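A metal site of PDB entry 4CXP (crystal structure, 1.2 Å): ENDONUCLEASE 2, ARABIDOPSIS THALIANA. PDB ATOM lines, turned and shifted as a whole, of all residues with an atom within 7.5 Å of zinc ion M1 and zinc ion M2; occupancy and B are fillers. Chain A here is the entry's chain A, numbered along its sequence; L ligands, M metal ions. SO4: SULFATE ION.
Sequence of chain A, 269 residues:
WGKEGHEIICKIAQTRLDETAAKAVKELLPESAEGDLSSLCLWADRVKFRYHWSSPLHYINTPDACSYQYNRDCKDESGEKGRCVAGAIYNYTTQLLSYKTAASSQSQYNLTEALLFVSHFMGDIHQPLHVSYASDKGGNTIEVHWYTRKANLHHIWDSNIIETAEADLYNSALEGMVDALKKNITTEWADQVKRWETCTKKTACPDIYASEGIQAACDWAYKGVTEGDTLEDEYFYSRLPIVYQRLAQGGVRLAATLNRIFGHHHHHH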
ATOM      1  N   TRP A   1      -8.792 -21.134 -16.482  1.00  0.00           N
ATOM      2  CA  TRP A   1     -10.114 -20.548 -16.170  1.00  0.00           C
ATOM      3  C   TRP A   1     -10.420 -20.751 -14.705  1.00  0.00           C
ATOM      4  O   TRP A   1      -9.899 -21.679 -14.084  1.00  0.00           O
ATOM      5  CB  TRP A   1     -11.233 -21.231 -16.967  1.00  0.00           C
ATOM      6  CG  TRP A   1     -11.029 -21.279 -18.463  1.00  0.00           C
ATOM      7  CD1 TRP A   1     -10.547 -22.325 -19.160  1.00  0.00           C
ATOM      8  CD2 TRP A   1     -11.313 -20.253 -19.423  1.00  0.00           C
ATOM      9  NE1 TRP A   1     -10.516 -22.032 -20.494  1.00  0.00           N
ATOM     10  CE2 TRP A   1     -10.986 -20.760 -20.684  1.00  0.00           C
ATOM     11  CE3 TRP A   1     -11.810 -18.949 -19.335  1.00  0.00           C
ATOM     12  CZ2 TRP A   1     -11.146 -20.020 -21.843  1.00  0.00           C
ATOM     13  CZ3 TRP A   1     -11.962 -18.210 -20.501  1.00  0.00           C
ATOM     14  CH2 TRP A   1     -11.635 -18.750 -21.731  1.00  0.00           C
ATOM     15  N   GLY A   2     -11.337 -19.946 -14.194  1.00  0.00           N
ATOM     16  CA  GLY A   2     -11.978 -20.224 -12.919  1.00  0.00           C
ATOM     17  C   GLY A   2     -13.052 -21.277 -13.038  1.00  0.00           C
ATOM     18  O   GLY A   2     -13.196 -21.973 -14.052  1.00  0.00           O
ATOM     19  N   LYS A   3     -13.838 -21.414 -11.986  1.00  0.00           N
ATOM     20  CA  LYS A   3     -14.788 -22.483 -11.873  1.00  0.00           C
ATOM     21  C   LYS A   3     -15.768 -22.510 -13.021  1.00  0.00           C
ATOM     22  O   LYS A   3     -16.074 -23.570 -13.570  1.00  0.00           O
ATOM     23  CB  LYS A   3     -15.542 -22.344 -10.540  1.00  0.00           C
ATOM     24  CG  LYS A   3     -16.694 -23.300 -10.341  1.00  0.00           C
ATOM     25  CD  LYS A   3     -17.403 -23.009  -9.022  1.00  0.00           C
ATOM     26  CE  LYS A   3     -18.487 -24.022  -8.697  1.00  0.00           C
ATOM     27  NZ  LYS A   3     -19.805 -23.625  -9.279  1.00  0.00           N
ATOM     28  N   GLY A   5     -15.686 -21.318 -16.134  1.00  0.00           N
ATOM     29  CA  GLY A   5     -15.165 -21.713 -17.429  1.00  0.00           C
ATOM     30  C   GLY A   5     -14.953 -23.203 -17.535  1.00  0.00           C
ATOM     31  O   GLY A   5     -15.298 -23.819 -18.541  1.00  0.00           O
ATOM     32  N   HIS A   6     -14.336 -23.808 -16.506  1.00  0.00           N
ATOM     33  CA  HIS A   6     -14.141 -25.258 -16.535  1.00  0.00           C
ATOM     34  C   HIS A   6     -15.461 -26.017 -16.531  1.00  0.00           C
ATOM     35  O   HIS A   6     -15.591 -27.044 -17.193  1.00  0.00           O
ATOM     36  CB  HIS A   6     -13.254 -25.724 -15.386  1.00  0.00           C
ATOM     37  CG  HIS A   6     -11.839 -25.330 -15.581  1.00  0.00           C
ATOM     38  ND1 HIS A   6     -11.016 -25.933 -16.510  1.00  0.00           N
ATOM     39  CD2 HIS A   6     -11.115 -24.320 -15.043  1.00  0.00           C
ATOM     40  CE1 HIS A   6      -9.846 -25.306 -16.506  1.00  0.00           C
ATOM     41  NE2 HIS A   6      -9.875 -24.324 -15.631  1.00  0.00           N
ATOM     42  N   CYS A  41     -14.079 -30.667 -12.471  1.00  0.00           N
ATOM     43  CA  CYS A  41     -13.167 -30.076 -13.461  1.00  0.00           C
ATOM     44  C   CYS A  41     -12.299 -28.939 -12.909  1.00  0.00           C
ATOM     45  O   CYS A  41     -11.474 -28.433 -13.654  1.00  0.00           O
ATOM     46  CB  CYS A  41     -13.883 -29.701 -14.784  1.00  0.00           C
ATOM     47  SG  CYS A  41     -14.146 -31.185 -15.778  1.00  0.00           S
ATOM     48  N   LEU A  42     -12.400 -28.645 -11.617  1.00  0.00           N
ATOM     49  CA  LEU A  42     -11.446 -27.783 -10.899  1.00  0.00           C
ATOM     50  C   LEU A  42     -10.532 -28.556  -9.956  1.00  0.00           C
ATOM     51  O   LEU A  42      -9.664 -27.963  -9.308  1.00  0.00           O
ATOM     52  CB  LEU A  42     -12.163 -26.648 -10.144  1.00  0.00           C
ATOM     53  CG  LEU A  42     -11.567 -25.241 -10.241  1.00  0.00           C
ATOM     54  CD1 LEU A  42     -11.495 -24.706 -11.644  1.00  0.00           C
ATOM     55  CD2 LEU A  42     -12.370 -24.308  -9.354  1.00  0.00           C
ATOM     56  N   ALA A  44      -7.927 -30.257 -10.481  1.00  0.00           N
ATOM     57  CA  ALA A  44      -6.511 -30.042 -10.713  1.00  0.00           C
ATOM     58  C   ALA A  44      -6.012 -28.769 -10.028  1.00  0.00           C
ATOM     59  O   ALA A  44      -4.882 -28.706  -9.561  1.00  0.00           O
ATOM     60  CB  ALA A  44      -6.197 -30.012 -12.195  1.00  0.00           C
ATOM     61  N   ASP A  45      -6.833 -27.729 -10.018  1.00  0.00           N
ATOM     62  CA  ASP A  45      -6.404 -26.509  -9.325  1.00  0.00           C
ATOM     63  C   ASP A  45      -6.222 -26.734  -7.820  1.00  0.00           C
ATOM     64  O   ASP A  45      -5.385 -26.066  -7.222  1.00  0.00           O
ATOM     65  CB  ASP A  45      -7.400 -25.368  -9.548  1.00  0.00           C
ATOM     66  CG  ASP A  45      -7.181 -24.608 -10.818  1.00  0.00           C
ATOM     67  OD1 ASP A  45      -6.209 -24.809 -11.546  1.00  0.00           O
ATOM     68  OD2 ASP A  45      -8.063 -23.763 -11.082  1.00  0.00           O
ATOM     69  N   ARG A  46      -6.953 -27.677  -7.260  1.00  0.00           N
ATOM     70  CA  ARG A  46      -6.922 -27.961  -5.826  1.00  0.00           C
ATOM     71  C   ARG A  46      -5.786 -28.893  -5.406  1.00  0.00           C
ATOM     72  O   ARG A  46      -5.668 -29.193  -4.233  1.00  0.00           O
ATOM     73  CB  ARG A  46      -8.255 -28.540  -5.365  1.00  0.00           C
ATOM     74  CG  ARG A  46      -9.383 -27.539  -5.437  1.00  0.00           C
ATOM     75  CD  ARG A  46     -10.603 -28.040  -4.669  1.00  0.00           C
ATOM     76  NE  ARG A  46     -11.184 -29.232  -5.274  1.00  0.00           N
ATOM     77  CZ  ARG A  46     -11.042 -30.471  -4.818  1.00  0.00           C
ATOM     78  NH1 ARG A  46     -10.337 -30.730  -3.712  1.00  0.00           N
ATOM     79  NH2 ARG A  46     -11.632 -31.455  -5.467  1.00  0.00           N
ATOM     80  N   LYS A  48      -2.537 -28.096  -6.758  1.00  0.00           N
ATOM     81  CA  LYS A  48      -1.358 -27.308  -7.123  1.00  0.00           C
ATOM     82  C   LYS A  48      -0.264 -27.311  -6.085  1.00  0.00           C
ATOM     83  O   LYS A  48       0.904 -27.157  -6.438  1.00  0.00           O
ATOM     84  CB  LYS A  48      -1.741 -25.848  -7.456  1.00  0.00           C
ATOM     85  CG  LYS A  48      -2.330 -25.675  -8.832  1.00  0.00           C
ATOM     86  CD  LYS A  48      -2.774 -24.234  -9.041  1.00  0.00           C
ATOM     87  CE  LYS A  48      -3.337 -24.019 -10.437  1.00  0.00           C
ATOM     88  NZ  LYS A  48      -3.914 -22.656 -10.572  1.00  0.00           N
ATOM     89  N   SER A  55       2.006 -27.634 -10.684  1.00  0.00           N
ATOM     90  CA  SER A  55       1.652 -26.232 -10.832  1.00  0.00           C
ATOM     91  C   SER A  55       2.014 -25.670 -12.222  1.00  0.00           C
ATOM     92  O   SER A  55       1.187 -25.011 -12.846  1.00  0.00           O
ATOM     93  CB  SER A  55       2.190 -25.395  -9.662  1.00  0.00           C
ATOM     94  OG  SER A  55       1.277 -25.375  -8.566  1.00  0.00           O
ATOM     95  N   LEU A  57       2.088 -27.143 -14.965  1.00  0.00           N
ATOM     96  CA  LEU A  57       1.348 -27.851 -15.993  1.00  0.00           C
ATOM     97  C   LEU A  57       0.060 -27.159 -16.410  1.00  0.00           C
ATOM     98  O   LEU A  57      -0.599 -27.630 -17.330  1.00  0.00           O
ATOM     99  CB  LEU A  57       1.037 -29.288 -15.522  1.00  0.00           C
ATOM    100  CG  LEU A  57       2.249 -30.127 -15.122  1.00  0.00           C
ATOM    101  CD1 LEU A  57       1.782 -31.526 -14.749  1.00  0.00           C
ATOM    102  CD2 LEU A  57       3.341 -30.176 -16.181  1.00  0.00           C
ATOM    103  N   HIS A  58      -0.297 -26.057 -15.751  1.00  0.00           N
ATOM    104  CA  HIS A  58      -1.534 -25.344 -16.094  1.00  0.00           C
ATOM    105  C   HIS A  58      -1.358 -24.327 -17.208  1.00  0.00           C
ATOM    106  O   HIS A  58      -2.353 -23.816 -17.715  1.00  0.00           O
ATOM    107  CB  HIS A  58      -2.112 -24.642 -14.871  1.00  0.00           C
ATOM    108  CG  HIS A  58      -2.590 -25.601 -13.830  1.00  0.00           C
ATOM    109  ND1 HIS A  58      -3.915 -25.722 -13.477  1.00  0.00           N
ATOM    110  CD2 HIS A  58      -1.901 -26.510 -13.104  1.00  0.00           C
ATOM    111  CE1 HIS A  58      -4.011 -26.688 -12.569  1.00  0.00           C
ATOM    112  NE2 HIS A  58      -2.804 -27.179 -12.319  1.00  0.00           N
ATOM    113  N   TYR A  59      -0.119 -24.013 -17.608  1.00  0.00           N
ATOM    114  CA  TYR A  59       0.094 -22.902 -18.529  1.00  0.00           C
ATOM    115  C   TYR A  59       1.324 -23.141 -19.381  1.00  0.00           C
ATOM    116  O   TYR A  59       2.039 -24.136 -19.234  1.00  0.00           O
ATOM    117  CB  TYR A  59       0.172 -21.570 -17.725  1.00  0.00           C
ATOM    118  CG  TYR A  59       1.269 -21.587 -16.698  1.00  0.00           C
ATOM    119  CD1 TYR A  59       2.603 -21.313 -17.043  1.00  0.00           C
ATOM    120  CD2 TYR A  59       1.001 -21.929 -15.378  1.00  0.00           C
ATOM    121  CE1 TYR A  59       3.600 -21.361 -16.094  1.00  0.00           C
ATOM    122  CE2 TYR A  59       2.013 -21.988 -14.442  1.00  0.00           C
ATOM    123  CZ  TYR A  59       3.309 -21.703 -14.796  1.00  0.00           C
ATOM    124  OH  TYR A  59       4.302 -21.773 -13.849  1.00  0.00           O
ATOM    125  N   VAL A  85       1.350 -26.991 -20.040  1.00  0.00           N
ATOM    126  CA  VAL A  85       0.023 -27.571 -20.256  1.00  0.00           C
ATOM    127  C   VAL A  85      -0.037 -28.454 -21.503  1.00  0.00           C
ATOM    128  O   VAL A  85      -0.777 -29.441 -21.504  1.00  0.00           O
ATOM    129  CB  VAL A  85      -1.072 -26.477 -20.208  1.00  0.00           C
ATOM    130  CG1 VAL A  85      -0.999 -25.501 -21.361  1.00  0.00           C
ATOM    131  CG2 VAL A  85      -2.439 -27.080 -20.071  1.00  0.00           C
ATOM    132  N   HIS A 120      -9.255 -30.763 -17.100  1.00  0.00           N
ATOM    133  CA  HIS A 120      -8.891 -29.421 -16.676  1.00  0.00           C
ATOM    134  C   HIS A 120      -7.901 -28.776 -17.639  1.00  0.00           C
ATOM    135  O   HIS A 120      -8.061 -27.615 -18.021  1.00  0.00           O
ATOM    136  CB  HIS A 120      -8.284 -29.476 -15.268  1.00  0.00           C
ATOM    137  CG  HIS A 120      -7.992 -28.129 -14.705  1.00  0.00           C
ATOM    138  ND1 HIS A 120      -8.902 -27.417 -13.968  1.00  0.00           N
ATOM    139  CD2 HIS A 120      -6.869 -27.366 -14.746  1.00  0.00           C
ATOM    140  CE1 HIS A 120      -8.365 -26.262 -13.610  1.00  0.00           C
ATOM    141  NE2 HIS A 120      -7.125 -26.214 -14.051  1.00  0.00           N
ATOM    142  N   PHE A 121      -6.859 -29.507 -18.011  1.00  0.00           N
ATOM    143  CA  PHE A 121      -5.814 -28.934 -18.858  1.00  0.00           C
ATOM    144  C   PHE A 121      -6.296 -28.649 -20.282  1.00  0.00           C
ATOM    145  O   PHE A 121      -5.869 -27.668 -20.873  1.00  0.00           O
ATOM    146  CB  PHE A 121      -4.570 -29.836 -18.851  1.00  0.00           C
ATOM    147  CG  PHE A 121      -3.878 -29.905 -17.513  1.00  0.00           C
ATOM    148  CD1 PHE A 121      -3.812 -28.818 -16.669  1.00  0.00           C
ATOM    149  CD2 PHE A 121      -3.254 -31.079 -17.116  1.00  0.00           C
ATOM    150  CE1 PHE A 121      -3.160 -28.907 -15.449  1.00  0.00           C
ATOM    151  CE2 PHE A 121      -2.609 -31.171 -15.902  1.00  0.00           C
ATOM    152  CZ  PHE A 121      -2.566 -30.080 -15.067  1.00  0.00           C
ATOM    153  N   GLY A 123      -9.151 -27.515 -20.844  1.00  0.00           N
ATOM    154  CA  GLY A 123      -9.690 -26.211 -20.616  1.00  0.00           C
ATOM    155  C   GLY A 123      -8.654 -25.120 -20.523  1.00  0.00           C
ATOM    156  O   GLY A 123      -8.736 -24.096 -21.218  1.00  0.00           O
ATOM    157  N   ASP A 124      -7.647 -25.300 -19.676  1.00  0.00           N
ATOM    158  CA  ASP A 124      -6.653 -24.257 -19.466  1.00  0.00           C
ATOM    159  C   ASP A 124      -5.920 -23.888 -20.745  1.00  0.00           C
ATOM    160  O   ASP A 124      -5.610 -22.726 -20.953  1.00  0.00           O
ATOM    161  CB  ASP A 124      -5.683 -24.630 -18.343  1.00  0.00           C
ATOM    162  CG  ASP A 124      -6.151 -24.221 -16.957  1.00  0.00           C
ATOM    163  OD1 ASP A 124      -7.236 -23.623 -16.878  1.00  0.00           O
ATOM    164  OD2 ASP A 124      -5.414 -24.509 -16.012  1.00  0.00           O
ATOM    165  N   ILE A 125      -5.605 -24.860 -21.624  1.00  0.00           N
ATOM    166  CA  ILE A 125      -4.873 -24.548 -22.843  1.00  0.00           C
ATOM    167  C   ILE A 125      -5.694 -23.695 -23.787  1.00  0.00           C
ATOM    168  O   ILE A 125      -5.139 -23.151 -24.740  1.00  0.00           O
ATOM    169  CB  ILE A 125      -4.317 -25.807 -23.517  1.00  0.00           C
ATOM    170  CG1 ILE A 125      -3.147 -25.472 -24.429  1.00  0.00           C
ATOM    171  CG2 ILE A 125      -5.417 -26.573 -24.247  1.00  0.00           C
ATOM    172  CD1 ILE A 125      -2.382 -26.701 -24.878  1.00  0.00           C
ATOM    173  N   GLN A 127      -7.563 -21.027 -22.513  1.00  0.00           N
ATOM    174  CA  GLN A 127      -7.623 -19.681 -21.941  1.00  0.00           C
ATOM    175  C   GLN A 127      -6.448 -18.913 -22.558  1.00  0.00           C
ATOM    176  O   GLN A 127      -5.297 -19.306 -22.372  1.00  0.00           O
ATOM    177  CB  GLN A 127      -7.518 -19.787 -20.411  1.00  0.00           C
ATOM    178  CG  GLN A 127      -8.183 -18.681 -19.605  1.00  0.00           C
ATOM    179  CD  GLN A 127      -7.445 -17.354 -19.598  1.00  0.00           C
ATOM    180  OE1 GLN A 127      -7.204 -16.775 -20.662  1.00  0.00           O
ATOM    181  NE2 GLN A 127      -7.107 -16.850 -18.421  1.00  0.00           N
ATOM    182  N   HIS A 130      -3.386 -18.286 -20.514  1.00  0.00           N
ATOM    183  CA  HIS A 130      -2.604 -19.458 -20.104  1.00  0.00           C
ATOM    184  C   HIS A 130      -1.531 -19.837 -21.120  1.00  0.00           C
ATOM    185  O   HIS A 130      -0.788 -20.751 -20.857  1.00  0.00           O
ATOM    186  CB  HIS A 130      -3.515 -20.646 -19.803  1.00  0.00           C
ATOM    187  CG  HIS A 130      -4.102 -20.589 -18.426  1.00  0.00           C
ATOM    188  ND1 HIS A 130      -3.887 -21.549 -17.484  1.00  0.00           N
ATOM    189  CD2 HIS A 130      -4.852 -19.638 -17.810  1.00  0.00           C
ATOM    190  CE1 HIS A 130      -4.467 -21.201 -16.352  1.00  0.00           C
ATOM    191  NE2 HIS A 130      -5.062 -20.032 -16.527  1.00  0.00           N
ATOM    192  N   HIS A 154      -5.134 -11.331 -16.023  1.00  0.00           N
ATOM    193  CA  HIS A 154      -5.301 -12.763 -16.040  1.00  0.00           C
ATOM    194  C   HIS A 154      -6.643 -13.193 -15.423  1.00  0.00           C
ATOM    195  O   HIS A 154      -7.373 -14.011 -15.986  1.00  0.00           O
ATOM    196  CB  HIS A 154      -4.119 -13.461 -15.348  1.00  0.00           C
ATOM    197  CG  HIS A 154      -4.177 -14.940 -15.492  1.00  0.00           C
ATOM    198  ND1 HIS A 154      -3.443 -15.615 -16.429  1.00  0.00           N
ATOM    199  CD2 HIS A 154      -4.944 -15.865 -14.885  1.00  0.00           C
ATOM    200  CE1 HIS A 154      -3.732 -16.901 -16.370  1.00  0.00           C
ATOM    201  NE2 HIS A 154      -4.669 -17.081 -15.444  1.00  0.00           N
ATOM    202  N   ASP A 158      -9.758 -15.385 -16.652  1.00  0.00           N
ATOM    203  CA  ASP A 158     -10.167 -16.613 -15.975  1.00  0.00           C
ATOM    204  C   ASP A 158     -11.634 -16.545 -15.529  1.00  0.00           C
ATOM    205  O   ASP A 158     -12.330 -17.567 -15.608  1.00  0.00           O
ATOM    206  CB  ASP A 158      -9.339 -16.867 -14.710  1.00  0.00           C
ATOM    207  CG  ASP A 158      -8.040 -17.622 -14.930  1.00  0.00           C
ATOM    208  OD1 ASP A 158      -7.804 -18.210 -16.006  1.00  0.00           O
ATOM    209  OD2 ASP A 158      -7.243 -17.667 -13.951  1.00  0.00           O
HETATM  210  S   SO4 L   1      -6.406 -21.866 -13.296  1.00  0.00           S
HETATM  211  O1  SO4 L   1      -6.955 -21.648 -11.899  1.00  0.00           O
HETATM  212  O2  SO4 L   1      -4.930 -22.427 -13.212  1.00  0.00           O
HETATM  213  O3  SO4 L   1      -6.667 -20.573 -14.038  1.00  0.00           O
HETATM  214  O4  SO4 L   1      -7.203 -22.975 -13.908  1.00  0.00           O
HETATM  215 ZN    ZN M   1      -5.712 -24.541 -13.876  1.00  0.00          ZN
HETATM  216 ZN    ZN M   2      -8.479 -22.896 -15.378  1.00  0.00          ZN
HETATM  217 ZN    ZN M   3      -5.700 -18.885 -14.849  1.00  0.00          ZN
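Zinc ion M2 is bound by an oxygen (O4) of the ligand (1.9 Å), a ring nitrogen (NE2) of His 6 (2.0 Å), the side-chain carboxylate (OD1) of Asp 124 (2.1 Å), the backbone nitrogen (N) of Trp 1 (2.1 Å) and the backbone carbonyl oxygen (O) of Trp 1 (2.3 Å).
Of the 25 residues printed, 4 come within 4 Å of zinc ion M1.
The side-chain carboxylate (OD2) of Asp 124 binds zinc ion M1 (2.2 Å).
O4 of the ligand is bound to zinc ion M1, 2.2 Å away.
Zinc ion M1 is bound by ND1 of His 58 (2.2 Å).
A ring nitrogen (NE2) of His 120 is bound to zinc ion M1, 2.2 Å away.
Zinc ion M1 is bound by an oxygen (O2) of the ligand (2.3 Å).
The side-chain carboxylate (OD1) of Asp 45 binds zinc ion M1 (2.4 Å).
Zinc ion M1 has six donor atoms within binding distance.
Of the 25 residues printed, 4 come within 4 Å of zinc ion M2.
NE1 of Trp 1 lies within hydrogen-bond range of O of Gly 123, 2.8 Å away.
O of His 58 is in hydrogen-bond range of ND1 of His 130, 2.7 Å away.
ND1 of His 120 sits at hydrogen-bond distance from O of Cys 41 (2.8 Å).
OD1 of Asp 45 sits close to NZ of Lys 48, 3.3 Å away.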
